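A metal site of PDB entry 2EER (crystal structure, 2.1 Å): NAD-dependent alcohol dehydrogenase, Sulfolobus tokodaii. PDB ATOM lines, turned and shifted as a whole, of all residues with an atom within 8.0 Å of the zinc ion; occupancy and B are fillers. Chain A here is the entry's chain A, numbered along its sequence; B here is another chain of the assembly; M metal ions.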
ATOM      1  N   GLU A  96     -21.784   1.820  20.477  1.00  0.00           N
ATOM      2  CA  GLU A  96     -22.897   2.358  19.705  1.00  0.00           C
ATOM      3  C   GLU A  96     -23.845   3.332  20.404  1.00  0.00           C
ATOM      4  O   GLU A  96     -24.147   3.199  21.587  1.00  0.00           O
ATOM      5  CB  GLU A  96     -23.678   1.172  19.142  1.00  0.00           C
ATOM      6  CG  GLU A  96     -22.786   0.244  18.304  1.00  0.00           C
ATOM      7  CD  GLU A  96     -23.379  -1.145  18.102  1.00  0.00           C
ATOM      8  OE1 GLU A  96     -24.605  -1.302  18.303  1.00  0.00           O
ATOM      9  OE2 GLU A  96     -22.620  -2.064  17.734  1.00  0.00           O
ATOM     10  N   GLY A  97     -24.323   4.323  19.633  1.00  0.00           N
ATOM     11  CA  GLY A  97     -25.241   5.327  20.162  1.00  0.00           C
ATOM     12  C   GLY A  97     -26.581   5.311  19.449  1.00  0.00           C
ATOM     13  O   GLY A  97     -26.727   4.651  18.423  1.00  0.00           O
ATOM     14  N   GLU A  98     -27.550   6.064  19.969  1.00  0.00           N
ATOM     15  CA  GLU A  98     -28.889   6.101  19.380  1.00  0.00           C
ATOM     16  C   GLU A  98     -29.117   7.169  18.298  1.00  0.00           C
ATOM     17  O   GLU A  98     -30.115   7.123  17.582  1.00  0.00           O
ATOM     18  CB  GLU A  98     -29.935   6.224  20.480  1.00  0.00           C
ATOM     19  CG  GLU A  98     -29.633   7.301  21.498  1.00  0.00           C
ATOM     20  CD  GLU A  98     -29.760   8.685  20.919  1.00  0.00           C
ATOM     21  OE1 GLU A  98     -30.656   8.889  20.062  1.00  0.00           O
ATOM     22  OE2 GLU A  98     -28.972   9.568  21.306  1.00  0.00           O
ATOM     23  N   GLY A  99     -28.206   8.140  18.201  1.00  0.00           N
ATOM     24  CA  GLY A  99     -28.315   9.162  17.160  1.00  0.00           C
ATOM     25  C   GLY A  99     -28.976  10.506  17.419  1.00  0.00           C
ATOM     26  O   GLY A  99     -28.672  11.480  16.710  1.00  0.00           O
ATOM     27  N   ASN A 100     -29.855  10.587  18.403  1.00  0.00           N
ATOM     28  CA  ASN A 100     -30.574  11.830  18.692  1.00  0.00           C
ATOM     29  C   ASN A 100     -29.952  12.777  19.721  1.00  0.00           C
ATOM     30  O   ASN A 100     -30.175  13.986  19.653  1.00  0.00           O
ATOM     31  CB  ASN A 100     -32.015  11.503  19.127  1.00  0.00           C
ATOM     32  CG  ASN A 100     -32.877  12.736  19.302  1.00  0.00           C
ATOM     33  OD1 ASN A 100     -33.118  13.484  18.357  1.00  0.00           O
ATOM     34  ND2 ASN A 100     -33.328  12.960  20.527  1.00  0.00           N
ATOM     35  N   CYS A 101     -29.176  12.250  20.670  1.00  0.00           N
ATOM     36  CA  CYS A 101     -28.584  13.107  21.698  1.00  0.00           C
ATOM     37  C   CYS A 101     -27.442  13.981  21.189  1.00  0.00           C
ATOM     38  O   CYS A 101     -26.888  13.732  20.110  1.00  0.00           O
ATOM     39  CB  CYS A 101     -28.087  12.261  22.875  1.00  0.00           C
ATOM     40  SG  CYS A 101     -26.463  11.538  22.599  1.00  0.00           S
ATOM     41  N   TYR A 102     -27.099  14.988  21.980  1.00  0.00           N
ATOM     42  CA  TYR A 102     -26.028  15.930  21.656  1.00  0.00           C
ATOM     43  C   TYR A 102     -24.759  15.260  21.148  1.00  0.00           C
ATOM     44  O   TYR A 102     -24.214  15.649  20.128  1.00  0.00           O
ATOM     45  CB  TYR A 102     -25.687  16.763  22.899  1.00  0.00           C
ATOM     46  CG  TYR A 102     -24.412  17.588  22.765  1.00  0.00           C
ATOM     47  CD1 TYR A 102     -24.414  18.817  22.109  1.00  0.00           C
ATOM     48  CD2 TYR A 102     -23.193  17.100  23.249  1.00  0.00           C
ATOM     49  CE1 TYR A 102     -23.237  19.563  21.947  1.00  0.00           C
ATOM     50  CE2 TYR A 102     -22.011  17.827  23.096  1.00  0.00           C
ATOM     51  CZ  TYR A 102     -22.037  19.053  22.436  1.00  0.00           C
ATOM     52  OH  TYR A 102     -20.869  19.763  22.277  1.00  0.00           O
ATOM     53  N   TYR A 103     -24.298  14.248  21.882  1.00  0.00           N
ATOM     54  CA  TYR A 103     -23.077  13.551  21.528  1.00  0.00           C
ATOM     55  C   TYR A 103     -23.124  12.774  20.209  1.00  0.00           C
ATOM     56  O   TYR A 103     -22.144  12.752  19.469  1.00  0.00           O
ATOM     57  CB  TYR A 103     -22.663  12.660  22.712  1.00  0.00           C
ATOM     58  CG  TYR A 103     -22.308  13.503  23.915  1.00  0.00           C
ATOM     59  CD1 TYR A 103     -21.095  14.197  23.968  1.00  0.00           C
ATOM     60  CD2 TYR A 103     -23.216  13.683  24.965  1.00  0.00           C
ATOM     61  CE1 TYR A 103     -20.800  15.055  25.022  1.00  0.00           C
ATOM     62  CE2 TYR A 103     -22.930  14.542  26.023  1.00  0.00           C
ATOM     63  CZ  TYR A 103     -21.721  15.223  26.040  1.00  0.00           C
ATOM     64  OH  TYR A 103     -21.448  16.090  27.071  1.00  0.00           O
ATOM     65  N   CYS A 104     -24.253  12.142  19.917  1.00  0.00           N
ATOM     66  CA  CYS A 104     -24.366  11.424  18.650  1.00  0.00           C
ATOM     67  C   CYS A 104     -24.357  12.443  17.507  1.00  0.00           C
ATOM     68  O   CYS A 104     -23.731  12.235  16.467  1.00  0.00           O
ATOM     69  CB  CYS A 104     -25.644  10.589  18.614  1.00  0.00           C
ATOM     70  SG  CYS A 104     -25.533   9.079  19.595  1.00  0.00           S
ATOM     71  N   ARG A 105     -25.043  13.570  17.716  1.00  0.00           N
ATOM     72  CA  ARG A 105     -25.100  14.614  16.694  1.00  0.00           C
ATOM     73  C   ARG A 105     -23.741  15.206  16.319  1.00  0.00           C
ATOM     74  O   ARG A 105     -23.512  15.572  15.165  1.00  0.00           O
ATOM     75  CB  ARG A 105     -26.037  15.738  17.122  1.00  0.00           C
ATOM     76  CG  ARG A 105     -27.518  15.346  17.113  1.00  0.00           C
ATOM     77  CD  ARG A 105     -28.390  16.430  17.724  1.00  0.00           C
ATOM     78  NE  ARG A 105     -29.776  15.975  17.865  1.00  0.00           N
ATOM     79  CZ  ARG A 105     -30.798  16.453  17.165  1.00  0.00           C
ATOM     80  NH1 ARG A 105     -30.618  17.416  16.262  1.00  0.00           N
ATOM     81  NH2 ARG A 105     -32.023  15.965  17.364  1.00  0.00           N
ATOM     82  N   GLU A 108     -19.721  11.902  18.295  1.00  0.00           N
ATOM     83  CA  GLU A 108     -19.052  11.290  19.435  1.00  0.00           C
ATOM     84  C   GLU A 108     -20.032  10.264  20.017  1.00  0.00           C
ATOM     85  O   GLU A 108     -20.386  10.319  21.197  1.00  0.00           O
ATOM     86  CB  GLU A 108     -18.721  12.361  20.489  1.00  0.00           C
ATOM     87  CG  GLU A 108     -17.759  13.447  19.991  1.00  0.00           C
ATOM     88  CD  GLU A 108     -16.347  12.926  19.776  1.00  0.00           C
ATOM     89  OE1 GLU A 108     -16.184  11.786  19.298  1.00  0.00           O
ATOM     90  OE2 GLU A 108     -15.392  13.657  20.083  1.00  0.00           O
ATOM     91  N   GLU A 109     -20.452   9.333  19.160  1.00  0.00           N
ATOM     92  CA  GLU A 109     -21.410   8.284  19.506  1.00  0.00           C
ATOM     93  C   GLU A 109     -21.122   7.469  20.758  1.00  0.00           C
ATOM     94  O   GLU A 109     -22.045   7.069  21.465  1.00  0.00           O
ATOM     95  CB  GLU A 109     -21.592   7.327  18.332  1.00  0.00           C
ATOM     96  CG  GLU A 109     -22.281   7.949  17.127  1.00  0.00           C
ATOM     97  CD  GLU A 109     -22.402   6.993  15.964  1.00  0.00           C
ATOM     98  OE1 GLU A 109     -22.954   5.886  16.157  1.00  0.00           O
ATOM     99  OE2 GLU A 109     -21.942   7.353  14.854  1.00  0.00           O
ATOM    100  N   HIS A 110     -19.843   7.214  21.013  1.00  0.00           N
ATOM    101  CA  HIS A 110     -19.476   6.423  22.176  1.00  0.00           C
ATOM    102  C   HIS A 110     -19.863   7.117  23.482  1.00  0.00           C
ATOM    103  O   HIS A 110     -19.970   6.475  24.520  1.00  0.00           O
ATOM    104  CB  HIS A 110     -17.973   6.110  22.149  1.00  0.00           C
ATOM    105  CG  HIS A 110     -17.105   7.329  22.216  1.00  0.00           C
ATOM    106  ND1 HIS A 110     -17.171   8.349  21.289  1.00  0.00           N
ATOM    107  CD2 HIS A 110     -16.114   7.668  23.085  1.00  0.00           C
ATOM    108  CE1 HIS A 110     -16.262   9.260  21.584  1.00  0.00           C
ATOM    109  NE2 HIS A 110     -15.607   8.875  22.664  1.00  0.00           N
ATOM    110  N   LEU A 111     -20.084   8.428  23.426  1.00  0.00           N
ATOM    111  CA  LEU A 111     -20.465   9.199  24.611  1.00  0.00           C
ATOM    112  C   LEU A 111     -21.971   9.456  24.650  1.00  0.00           C
ATOM    113  O   LEU A 111     -22.443  10.339  25.367  1.00  0.00           O
ATOM    114  CB  LEU A 111     -19.693  10.526  24.647  1.00  0.00           C
ATOM    115  CG  LEU A 111     -18.173  10.373  24.834  1.00  0.00           C
ATOM    116  CD1 LEU A 111     -17.502  11.724  24.706  1.00  0.00           C
ATOM    117  CD2 LEU A 111     -17.886   9.767  26.197  1.00  0.00           C
ATOM    118  N   CYS A 112     -22.710   8.677  23.881  1.00  0.00           N
ATOM    119  CA  CYS A 112     -24.161   8.781  23.813  1.00  0.00           C
ATOM    120  C   CYS A 112     -24.764   8.783  25.213  1.00  0.00           C
ATOM    121  O   CYS A 112     -24.248   8.123  26.117  1.00  0.00           O
ATOM    122  CB  CYS A 112     -24.727   7.613  23.005  1.00  0.00           C
ATOM    123  SG  CYS A 112     -26.525   7.530  22.935  1.00  0.00           S
ATOM    124  N   ASP A 113     -25.857   9.534  25.396  1.00  0.00           N
ATOM    125  CA  ASP A 113     -26.525   9.601  26.687  1.00  0.00           C
ATOM    126  C   ASP A 113     -27.265   8.294  26.981  1.00  0.00           C
ATOM    127  O   ASP A 113     -27.491   7.936  28.140  1.00  0.00           O
ATOM    128  CB  ASP A 113     -27.519  10.768  26.739  1.00  0.00           C
ATOM    129  CG  ASP A 113     -26.842  12.124  26.694  1.00  0.00           C
ATOM    130  OD1 ASP A 113     -25.729  12.251  27.239  1.00  0.00           O
ATOM    131  OD2 ASP A 113     -27.426  13.066  26.116  1.00  0.00           O
ATOM    132  N   SER A 114     -27.632   7.578  25.926  1.00  0.00           N
ATOM    133  CA  SER A 114     -28.325   6.312  26.064  1.00  0.00           C
ATOM    134  C   SER A 114     -27.498   5.283  25.313  1.00  0.00           C
ATOM    135  O   SER A 114     -27.958   4.703  24.331  1.00  0.00           O
ATOM    136  CB  SER A 114     -29.723   6.419  25.449  1.00  0.00           C
ATOM    137  OG  SER A 114     -30.455   7.469  26.073  1.00  0.00           O
ATOM    138  N   PRO A 115     -26.261   5.032  25.784  1.00  0.00           N
ATOM    139  CA  PRO A 115     -25.310   4.087  25.190  1.00  0.00           C
ATOM    140  C   PRO A 115     -25.751   2.647  25.023  1.00  0.00           C
ATOM    141  O   PRO A 115     -26.480   2.090  25.851  1.00  0.00           O
ATOM    142  CB  PRO A 115     -24.104   4.205  26.120  1.00  0.00           C
ATOM    143  CG  PRO A 115     -24.732   4.474  27.442  1.00  0.00           C
ATOM    144  CD  PRO A 115     -25.760   5.516  27.082  1.00  0.00           C
ATOM    145  N   ARG A 116     -25.292   2.055  23.926  1.00  0.00           N
ATOM    146  CA  ARG A 116     -25.574   0.672  23.588  1.00  0.00           C
ATOM    147  C   ARG A 116     -24.194   0.050  23.391  1.00  0.00           C
ATOM    148  O   ARG A 116     -23.719  -0.114  22.269  1.00  0.00           O
ATOM    149  CB  ARG A 116     -26.398   0.615  22.297  1.00  0.00           C
ATOM    150  CG  ARG A 116     -27.300  -0.596  22.158  1.00  0.00           C
ATOM    151  CD  ARG A 116     -28.410  -0.301  21.137  1.00  0.00           C
ATOM    152  NE  ARG A 116     -28.947   1.052  21.259  1.00  0.00           N
ATOM    153  CZ  ARG A 116     -29.408   1.782  20.245  1.00  0.00           C
ATOM    154  NH1 ARG A 116     -29.417   1.286  19.007  1.00  0.00           N
ATOM    155  NH2 ARG A 116     -29.865   3.005  20.457  1.00  0.00           N
ATOM    156  N   LYS B 263     -19.917  15.740  29.811  1.00  0.00           N
ATOM    157  CA  LYS B 263     -18.972  14.829  29.205  1.00  0.00           C
ATOM    158  C   LYS B 263     -18.187  15.599  28.161  1.00  0.00           C
ATOM    159  O   LYS B 263     -18.714  16.477  27.490  1.00  0.00           O
ATOM    160  CB  LYS B 263     -19.740  13.661  28.554  1.00  0.00           C
ATOM    161  CG  LYS B 263     -20.271  12.610  29.548  1.00  0.00           C
ATOM    162  CD  LYS B 263     -21.110  11.502  28.871  1.00  0.00           C
ATOM    163  CE  LYS B 263     -22.482  12.013  28.414  1.00  0.00           C
ATOM    164  NZ  LYS B 263     -23.258  10.943  27.803  1.00  0.00           N
HETATM  165 ZN    ZN M   1     -26.835   9.402  21.559  1.00  0.00          ZN
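OD1 of Asp 113 lies within salt-bridge range of NZ of Lys 263 of chain B (2.9 Å). NZ of Lys 263 of chain B lies within hydrogen-bond range of O of Cys 112. N of Gly 99 sits close to SG of Cys 104 (3.2 Å). The backbone NH (N) of Asn 100 is in hydrogen-bond range of the side-chain carboxylate (OE1) of Glu 98, 2.5 Å away. The side-chain sulfur (SG) of Cys 101 lies close to the backbone NH (N) of Asp 113 (3.5 Å). The side-chain sulfur (SG) of Cys 112 sits close to the backbone NH (N) of Ser 114 (3.2 Å). The backbone NH (N) of Tyr 103 lies close to the side-chain sulfur (SG) of Cys 101 (3.5 Å).
Gly 99 touches the zinc ion (N to ZN, 3.8 Å). N of Asp 113 touches the zinc ion (3.96 Å). Of the 20 residues printed, 6 come within 4 Å of the zinc ion.
OE2 of Glu 98 binds the zinc ion. The side-chain sulfur (SG) of Cys 112 binds the zinc ion (2.3 Å). SG of Cys 104 is bound to the zinc ion (2.4 Å). The zinc ion is bound by SG of Cys 101, 2.4 Å away.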
